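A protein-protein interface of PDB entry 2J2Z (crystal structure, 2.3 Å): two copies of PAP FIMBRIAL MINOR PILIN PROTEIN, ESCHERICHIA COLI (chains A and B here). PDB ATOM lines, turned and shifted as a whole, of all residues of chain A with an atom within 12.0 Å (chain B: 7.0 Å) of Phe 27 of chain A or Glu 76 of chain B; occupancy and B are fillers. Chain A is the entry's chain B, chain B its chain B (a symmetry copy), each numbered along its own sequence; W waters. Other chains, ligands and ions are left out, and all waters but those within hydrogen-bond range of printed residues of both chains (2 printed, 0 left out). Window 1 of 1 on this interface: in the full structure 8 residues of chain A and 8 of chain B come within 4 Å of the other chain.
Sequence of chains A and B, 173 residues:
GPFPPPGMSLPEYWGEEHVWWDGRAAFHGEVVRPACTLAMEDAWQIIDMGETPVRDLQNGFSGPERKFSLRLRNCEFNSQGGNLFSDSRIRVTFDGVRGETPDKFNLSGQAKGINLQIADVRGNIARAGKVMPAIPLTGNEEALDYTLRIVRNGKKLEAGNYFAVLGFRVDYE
Of the printed residues of chain B, Ala 26 of chain A touches Val 31.
Phe 27 of chain A touches just these residues of chain B: Val 31, Val 32, Arg 33 and Glu 76.
Of the printed residues of chain B, Glu 30 of chain A touches Glu 30.
Val 31 of chain A touches none of the printed residues of chain B.
Printed residues of chain A within 4 Å of Glu 30 of chain B: His 28 (3.5 Å) and Glu 30 (3.8 Å).
Val 31 of chain B touches just these residues of chain A: Ala 26 (3.8 Å), Phe 27 (3.2 Å) and His 28 (3.0 Å).
Val 32 of chain B touches just one residue of chain A: Phe 27.
Of chain A, only Phe 27 (3.3 Å) comes within 4 Å of Arg 33 of chain B.
No residue of chain A comes within 4 Å of Pro 34 of chain B.
No residue of chain A comes within 4 Å of Asn 74 of chain B.
No residue of chain A comes within 4 Å of Cys 75 of chain B.
Of chain A, only Phe 27 comes within 4 Å of Glu 76 of chain B.
No residue of chain A comes within 4 Å of Phe 77 of chain B.
No residue of chain A comes within 4 Å of Asn 78 of chain B.
Ser 79 of chain B touches none of the printed residues of chain A.
The nearest residue of chain B that does not touch Phe 27 of chain A is Pro 34 of chain B (4.6 Å).
The nearest printed residue of chain B that does not touch His 28 of chain A is Val 32 of chain B (5.1 Å).
Among the printed residues, merely in contact across the chains: Ala 26 of chain A with Val 31 of chain B (3.8 Å), Phe 27 of chain A with Val 31 of chain B (3.2 Å), Phe 27 of chain A with Val 32 of chain B (3.4 Å), Phe 27 of chain A with Arg 33 of chain B (3.3 Å), Phe 27 of chain A with Glu 76 of chain B (3.1 Å), His 28 of chain A with Glu 30 of chain B (3.5 Å) and Glu 30 of chain A with Glu 30 of chain B (3.8 Å).
Hydrophobic or aromatic side chains of chain A within 4 Å of the printed part of chain B: Phe 27.
Hydrophobic or aromatic side chains of chain B within 4 Å of the printed part of chain A: Val 31.
Among the printed residues, no Asp or Glu carboxylate lies within 4 Å of a Lys or Arg side-chain nitrogen of the other chain.
N of His 28 of chain A lies within hydrogen-bond range of O of Val 31 of chain B.
The side-chain sulfur (SG) of Cys 36 of chain B is disulfide-bonded to the side-chain sulfur (SG) of Cys 75 of chain B, 2.0 Å away.
NH1 of Arg 33 of chain B is in hydrogen-bond range of O of Cys 75 of chain B.
O of Ala 25 of chain A is in hydrogen-bond range of ND1 of His 28 of chain A (3.2 Å).
Glu 30 of chain B touches its own counterpart, Glu 30 of chain A.
Positions printed for both chains: 30 and 31.
Water W1 bridges the side-chain carboxylate of Glu 30 of chain A (2.8 Å) and the backbone NH of Glu 30 of chain B (3.0 Å).
Water W2 lies within hydrogen-bond range of the side-chain carboxylate (OE2) of Glu 30 of chain B (2.8 Å) and the backbone NH (N) of Glu 30 of chain A (3.0 Å).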
ATOM      1  N   ARG A  24     -11.503  16.504  -6.455  1.00  0.00           N
ATOM      2  CA  ARG A  24     -12.185  15.181  -6.343  1.00  0.00           C
ATOM      3  C   ARG A  24     -13.705  15.353  -6.331  1.00  0.00           C
ATOM      4  O   ARG A  24     -14.340  15.468  -7.386  1.00  0.00           O
ATOM      5  CB  ARG A  24     -11.726  14.468  -5.068  1.00  0.00           C
ATOM      6  N   ALA A  25     -14.283  15.373  -5.133  1.00  0.00           N
ATOM      7  CA  ALA A  25     -15.724  15.534  -4.978  1.00  0.00           C
ATOM      8  C   ALA A  25     -16.143  16.957  -5.336  1.00  0.00           C
ATOM      9  O   ALA A  25     -15.528  17.921  -4.887  1.00  0.00           O
ATOM     10  CB  ALA A  25     -16.131  15.214  -3.548  1.00  0.00           C
ATOM     11  N   ALA A  26     -17.184  17.085  -6.151  1.00  0.00           N
ATOM     12  CA  ALA A  26     -17.675  18.397  -6.549  1.00  0.00           C
ATOM     13  C   ALA A  26     -18.447  19.064  -5.411  1.00  0.00           C
ATOM     14  O   ALA A  26     -18.468  20.290  -5.299  1.00  0.00           O
ATOM     15  CB  ALA A  26     -18.563  18.270  -7.775  1.00  0.00           C
ATOM     16  N   PHE A  27     -19.079  18.249  -4.569  1.00  0.00           N
ATOM     17  CA  PHE A  27     -19.861  18.754  -3.444  1.00  0.00           C
ATOM     18  C   PHE A  27     -19.359  18.185  -2.118  1.00  0.00           C
ATOM     19  O   PHE A  27     -19.353  16.967  -1.915  1.00  0.00           O
ATOM     20  CB  PHE A  27     -21.339  18.381  -3.612  1.00  0.00           C
ATOM     21  CG  PHE A  27     -21.927  18.770  -4.945  1.00  0.00           C
ATOM     22  CD1 PHE A  27     -22.319  17.791  -5.858  1.00  0.00           C
ATOM     23  CD2 PHE A  27     -22.096  20.108  -5.286  1.00  0.00           C
ATOM     24  CE1 PHE A  27     -22.871  18.145  -7.094  1.00  0.00           C
ATOM     25  CE2 PHE A  27     -22.647  20.470  -6.516  1.00  0.00           C
ATOM     26  CZ  PHE A  27     -23.035  19.483  -7.421  1.00  0.00           C
ATOM     27  N   HIS A  28     -18.946  19.061  -1.209  1.00  0.00           N
ATOM     28  CA  HIS A  28     -18.464  18.611   0.089  1.00  0.00           C
ATOM     29  C   HIS A  28     -18.385  19.746   1.091  1.00  0.00           C
ATOM     30  O   HIS A  28     -18.644  20.905   0.759  1.00  0.00           O
ATOM     31  CB  HIS A  28     -17.086  17.947  -0.035  1.00  0.00           C
ATOM     32  CG  HIS A  28     -16.025  18.848  -0.592  1.00  0.00           C
ATOM     33  ND1 HIS A  28     -15.829  19.018  -1.946  1.00  0.00           N
ATOM     34  CD2 HIS A  28     -15.106  19.631   0.023  1.00  0.00           C
ATOM     35  CE1 HIS A  28     -14.833  19.865  -2.139  1.00  0.00           C
ATOM     36  NE2 HIS A  28     -14.377  20.253  -0.962  1.00  0.00           N
ATOM     37  N   GLY A  29     -18.021  19.397   2.320  1.00  0.00           N
ATOM     38  CA  GLY A  29     -17.913  20.388   3.371  1.00  0.00           C
ATOM     39  C   GLY A  29     -16.653  21.233   3.329  1.00  0.00           C
ATOM     40  O   GLY A  29     -15.701  20.950   2.597  1.00  0.00           O
ATOM     41  N   GLU A  30     -16.675  22.285   4.135  1.00  0.00           N
ATOM     42  CA  GLU A  30     -15.574  23.224   4.268  1.00  0.00           C
ATOM     43  C   GLU A  30     -14.245  22.504   4.530  1.00  0.00           C
ATOM     44  O   GLU A  30     -14.178  21.593   5.353  1.00  0.00           O
ATOM     45  CB  GLU A  30     -15.902  24.187   5.420  1.00  0.00           C
ATOM     46  CG  GLU A  30     -14.848  25.224   5.749  1.00  0.00           C
ATOM     47  CD  GLU A  30     -15.380  26.306   6.680  1.00  0.00           C
ATOM     48  OE1 GLU A  30     -14.572  27.090   7.227  1.00  0.00           O
ATOM     49  OE2 GLU A  30     -16.613  26.382   6.861  1.00  0.00           O
ATOM     50  N   VAL A  31     -13.205  22.915   3.810  1.00  0.00           N
ATOM     51  CA  VAL A  31     -11.862  22.354   3.954  1.00  0.00           C
ATOM     52  C   VAL A  31     -10.899  23.538   4.100  1.00  0.00           C
ATOM     53  O   VAL A  31     -10.780  24.354   3.191  1.00  0.00           O
ATOM     54  CB  VAL A  31     -11.448  21.533   2.702  1.00  0.00           C
ATOM     55  CG1 VAL A  31     -10.081  20.884   2.931  1.00  0.00           C
ATOM     56  CG2 VAL A  31     -12.492  20.466   2.406  1.00  0.00           C
ATOM     57  N   GLU B  30     -17.972  25.274   2.131  1.00  0.00           N
ATOM     58  CA  GLU B  30     -18.948  24.250   1.792  1.00  0.00           C
ATOM     59  C   GLU B  30     -19.608  24.527   0.435  1.00  0.00           C
ATOM     60  O   GLU B  30     -20.003  25.656   0.149  1.00  0.00           O
ATOM     61  CB  GLU B  30     -20.004  24.207   2.906  1.00  0.00           C
ATOM     62  CG  GLU B  30     -21.142  23.225   2.714  1.00  0.00           C
ATOM     63  CD  GLU B  30     -21.957  23.036   3.988  1.00  0.00           C
ATOM     64  OE1 GLU B  30     -23.060  22.448   3.924  1.00  0.00           O
ATOM     65  OE2 GLU B  30     -21.490  23.469   5.062  1.00  0.00           O
ATOM     66  N   VAL B  31     -19.703  23.489  -0.392  1.00  0.00           N
ATOM     67  CA  VAL B  31     -20.327  23.574  -1.712  1.00  0.00           C
ATOM     68  C   VAL B  31     -21.320  22.409  -1.809  1.00  0.00           C
ATOM     69  O   VAL B  31     -20.923  21.250  -1.746  1.00  0.00           O
ATOM     70  CB  VAL B  31     -19.282  23.425  -2.850  1.00  0.00           C
ATOM     71  CG1 VAL B  31     -19.958  23.616  -4.210  1.00  0.00           C
ATOM     72  CG2 VAL B  31     -18.166  24.444  -2.672  1.00  0.00           C
ATOM     73  N   VAL B  32     -22.606  22.706  -1.961  1.00  0.00           N
ATOM     74  CA  VAL B  32     -23.596  21.639  -2.033  1.00  0.00           C
ATOM     75  C   VAL B  32     -24.402  21.635  -3.325  1.00  0.00           C
ATOM     76  O   VAL B  32     -24.503  22.649  -4.019  1.00  0.00           O
ATOM     77  CB  VAL B  32     -24.572  21.711  -0.828  1.00  0.00           C
ATOM     78  CG1 VAL B  32     -23.780  21.829   0.480  1.00  0.00           C
ATOM     79  CG2 VAL B  32     -25.527  22.882  -0.987  1.00  0.00           C
ATOM     80  N   ARG B  33     -24.967  20.483  -3.659  1.00  0.00           N
ATOM     81  CA  ARG B  33     -25.775  20.387  -4.863  1.00  0.00           C
ATOM     82  C   ARG B  33     -27.088  21.105  -4.614  1.00  0.00           C
ATOM     83  O   ARG B  33     -27.813  20.777  -3.682  1.00  0.00           O
ATOM     84  CB  ARG B  33     -26.080  18.925  -5.212  1.00  0.00           C
ATOM     85  CG  ARG B  33     -26.943  18.771  -6.477  1.00  0.00           C
ATOM     86  CD  ARG B  33     -27.616  17.415  -6.524  1.00  0.00           C
ATOM     87  NE  ARG B  33     -26.631  16.349  -6.400  1.00  0.00           N
ATOM     88  CZ  ARG B  33     -25.847  15.933  -7.387  1.00  0.00           C
ATOM     89  NH1 ARG B  33     -25.940  16.488  -8.589  1.00  0.00           N
ATOM     90  NH2 ARG B  33     -24.955  14.974  -7.160  1.00  0.00           N
ATOM     91  N   PRO B  34     -27.404  22.114  -5.427  1.00  0.00           N
ATOM     92  CA  PRO B  34     -28.684  22.781  -5.165  1.00  0.00           C
ATOM     93  C   PRO B  34     -29.840  21.958  -5.737  1.00  0.00           C
ATOM     94  O   PRO B  34     -29.610  21.013  -6.487  1.00  0.00           O
ATOM     95  CB  PRO B  34     -28.518  24.137  -5.847  1.00  0.00           C
ATOM     96  CG  PRO B  34     -27.555  23.855  -6.964  1.00  0.00           C
ATOM     97  CD  PRO B  34     -26.568  22.880  -6.372  1.00  0.00           C
ATOM     98  N   CYS B  36     -33.187  21.339  -8.090  1.00  0.00           N
ATOM     99  CA  CYS B  36     -33.441  21.763  -9.461  1.00  0.00           C
ATOM    100  C   CYS B  36     -34.467  22.879  -9.543  1.00  0.00           C
ATOM    101  O   CYS B  36     -35.384  22.955  -8.728  1.00  0.00           O
ATOM    102  CB  CYS B  36     -33.947  20.589 -10.305  1.00  0.00           C
ATOM    103  SG  CYS B  36     -32.994  19.048 -10.123  1.00  0.00           S
ATOM    104  N   LEU B  72     -35.166  20.702 -15.855  1.00  0.00           N
ATOM    105  CA  LEU B  72     -34.707  20.824 -14.477  1.00  0.00           C
ATOM    106  C   LEU B  72     -33.250  21.272 -14.500  1.00  0.00           C
ATOM    107  O   LEU B  72     -32.363  20.510 -14.882  1.00  0.00           O
ATOM    108  CB  LEU B  72     -34.857  19.488 -13.757  1.00  0.00           C
ATOM    109  CG  LEU B  72     -36.307  19.003 -13.660  1.00  0.00           C
ATOM    110  CD1 LEU B  72     -36.335  17.635 -13.011  1.00  0.00           C
ATOM    111  CD2 LEU B  72     -37.146  19.999 -12.848  1.00  0.00           C
ATOM    112  N   ARG B  73     -33.009  22.509 -14.080  1.00  0.00           N
ATOM    113  CA  ARG B  73     -31.666  23.076 -14.122  1.00  0.00           C
ATOM    114  C   ARG B  73     -31.015  23.403 -12.784  1.00  0.00           C
ATOM    115  O   ARG B  73     -31.649  23.363 -11.732  1.00  0.00           O
ATOM    116  CB  ARG B  73     -31.683  24.357 -14.960  1.00  0.00           C
ATOM    117  CG  ARG B  73     -32.718  24.375 -16.072  1.00  0.00           C
ATOM    118  CD  ARG B  73     -32.083  24.778 -17.390  1.00  0.00           C
ATOM    119  NE  ARG B  73     -31.337  26.031 -17.285  1.00  0.00           N
ATOM    120  CZ  ARG B  73     -30.449  26.450 -18.186  1.00  0.00           C
ATOM    121  NH1 ARG B  73     -30.193  25.715 -19.263  1.00  0.00           N
ATOM    122  NH2 ARG B  73     -29.811  27.602 -18.004  1.00  0.00           N
ATOM    123  N   ASN B  74     -29.731  23.740 -12.863  1.00  0.00           N
ATOM    124  CA  ASN B  74     -28.932  24.132 -11.710  1.00  0.00           C
ATOM    125  C   ASN B  74     -28.652  23.022 -10.703  1.00  0.00           C
ATOM    126  O   ASN B  74     -28.042  23.268  -9.661  1.00  0.00           O
ATOM    127  CB  ASN B  74     -29.608  25.302 -10.983  1.00  0.00           C
ATOM    128  CG  ASN B  74     -28.647  26.065 -10.089  1.00  0.00           C
ATOM    129  OD1 ASN B  74     -29.037  26.608  -9.048  1.00  0.00           O
ATOM    130  ND2 ASN B  74     -27.383  26.125 -10.498  1.00  0.00           N
ATOM    131  N   CYS B  75     -29.079  21.804 -10.998  1.00  0.00           N
ATOM    132  CA  CYS B  75     -28.862  20.719 -10.051  1.00  0.00           C
ATOM    133  C   CYS B  75     -27.983  19.600 -10.598  1.00  0.00           C
ATOM    134  O   CYS B  75     -27.947  18.514 -10.033  1.00  0.00           O
ATOM    135  CB  CYS B  75     -30.209  20.141  -9.615  1.00  0.00           C
ATOM    136  SG  CYS B  75     -31.210  19.497 -10.996  1.00  0.00           S
ATOM    137  N   GLU B  76     -27.261  19.879 -11.677  1.00  0.00           N
ATOM    138  CA  GLU B  76     -26.413  18.877 -12.311  1.00  0.00           C
ATOM    139  C   GLU B  76     -27.221  17.603 -12.504  1.00  0.00           C
ATOM    140  O   GLU B  76     -26.811  16.517 -12.103  1.00  0.00           O
ATOM    141  CB  GLU B  76     -25.157  18.616 -11.474  1.00  0.00           C
ATOM    142  CG  GLU B  76     -24.182  19.783 -11.534  1.00  0.00           C
ATOM    143  CD  GLU B  76     -22.777  19.423 -11.085  1.00  0.00           C
ATOM    144  OE1 GLU B  76     -22.260  18.374 -11.525  1.00  0.00           O
ATOM    145  OE2 GLU B  76     -22.178  20.198 -10.305  1.00  0.00           O
ATOM    146  N   PHE B  77     -28.385  17.783 -13.121  1.00  0.00           N
ATOM    147  CA  PHE B  77     -29.348  16.725 -13.421  1.00  0.00           C
ATOM    148  C   PHE B  77     -28.710  15.502 -14.073  1.00  0.00           C
ATOM    149  O   PHE B  77     -29.031  14.363 -13.725  1.00  0.00           O
ATOM    150  CB  PHE B  77     -30.435  17.294 -14.342  1.00  0.00           C
ATOM    151  CG  PHE B  77     -31.538  16.325 -14.681  1.00  0.00           C
ATOM    152  CD1 PHE B  77     -32.470  15.941 -13.722  1.00  0.00           C
ATOM    153  CD2 PHE B  77     -31.681  15.844 -15.979  1.00  0.00           C
ATOM    154  CE1 PHE B  77     -33.531  15.098 -14.052  1.00  0.00           C
ATOM    155  CE2 PHE B  77     -32.739  15.003 -16.319  1.00  0.00           C
ATOM    156  CZ  PHE B  77     -33.669  14.629 -15.353  1.00  0.00           C
ATOM    157  N   ASN B  78     -27.814  15.741 -15.024  1.00  0.00           N
ATOM    158  CA  ASN B  78     -27.144  14.653 -15.731  1.00  0.00           C
ATOM    159  C   ASN B  78     -25.791  14.315 -15.124  1.00  0.00           C
ATOM    160  O   ASN B  78     -25.026  15.208 -14.756  1.00  0.00           O
ATOM    161  CB  ASN B  78     -26.949  15.015 -17.208  1.00  0.00           C
ATOM    162  CG  ASN B  78     -28.256  15.059 -17.976  1.00  0.00           C
ATOM    163  OD1 ASN B  78     -28.959  14.054 -18.084  1.00  0.00           O
ATOM    164  ND2 ASN B  78     -28.588  16.228 -18.517  1.00  0.00           N
ATOM    165  N   SER B  79     -25.504  13.019 -15.029  1.00  0.00           N
ATOM    166  CA  SER B  79     -24.235  12.539 -14.490  1.00  0.00           C
ATOM    167  C   SER B  79     -23.553  11.674 -15.549  1.00  0.00           C
ATOM    168  O   SER B  79     -24.102  11.462 -16.632  1.00  0.00           O
ATOM    169  CB  SER B  79     -24.457  11.726 -13.204  1.00  0.00           C
ATOM    170  OG  SER B  79     -25.192  10.537 -13.442  1.00  0.00           O
ATOM    171  N   GLY B  82     -25.963   8.594 -16.157  1.00  0.00           N
ATOM    172  CA  GLY B  82     -27.370   8.657 -15.804  1.00  0.00           C
ATOM    173  C   GLY B  82     -27.849  10.053 -15.457  1.00  0.00           C
ATOM    174  O   GLY B  82     -27.216  11.048 -15.814  1.00  0.00           O
ATOM    175  N   ASN B  83     -28.980  10.120 -14.763  1.00  0.00           N
ATOM    176  CA  ASN B  83     -29.558  11.387 -14.348  1.00  0.00           C
ATOM    177  C   ASN B  83     -30.386  11.170 -13.090  1.00  0.00           C
ATOM    178  O   ASN B  83     -30.868  10.066 -12.832  1.00  0.00           O
ATOM    179  CB  ASN B  83     -30.451  11.965 -15.446  1.00  0.00           C
ATOM    180  CG  ASN B  83     -31.620  11.062 -15.777  1.00  0.00           C
ATOM    181  OD1 ASN B  83     -31.555  10.253 -16.711  1.00  0.00           O
ATOM    182  ND2 ASN B  83     -32.691  11.177 -15.000  1.00  0.00           N
ATOM    183  N   LEU B  84     -30.553  12.235 -12.319  1.00  0.00           N
ATOM    184  CA  LEU B  84     -31.318  12.191 -11.077  1.00  0.00           C
ATOM    185  C   LEU B  84     -32.647  11.442 -11.184  1.00  0.00           C
ATOM    186  O   LEU B  84     -33.006  10.673 -10.296  1.00  0.00           O
ATOM    187  CB  LEU B  84     -31.584  13.614 -10.589  1.00  0.00           C
ATOM    188  CG  LEU B  84     -30.371  14.487 -10.253  1.00  0.00           C
ATOM    189  CD1 LEU B  84     -30.852  15.862  -9.758  1.00  0.00           C
ATOM    190  CD2 LEU B  84     -29.532  13.806  -9.189  1.00  0.00           C
ATOM    191  N   GLU B 142     -31.556  17.429 -20.886  1.00  0.00           N
ATOM    192  CA  GLU B 142     -31.725  17.601 -19.452  1.00  0.00           C
ATOM    193  C   GLU B 142     -33.172  17.982 -19.151  1.00  0.00           C
ATOM    194  O   GLU B 142     -33.436  18.885 -18.359  1.00  0.00           O
ATOM    195  CB  GLU B 142     -30.763  18.689 -18.968  1.00  0.00           C
ATOM    196  CG  GLU B 142     -30.424  18.640 -17.493  1.00  0.00           C
ATOM    197  CD  GLU B 142     -29.142  19.391 -17.176  1.00  0.00           C
ATOM    198  OE1 GLU B 142     -29.119  20.631 -17.335  1.00  0.00           O
ATOM    199  OE2 GLU B 142     -28.156  18.736 -16.776  1.00  0.00           O
HETATM  200  O   HOH W   1     -18.301  26.791   4.660  1.00  0.00           O
HETATM  201  O   HOH W   2     -19.004  22.531   5.957  1.00  0.00           O
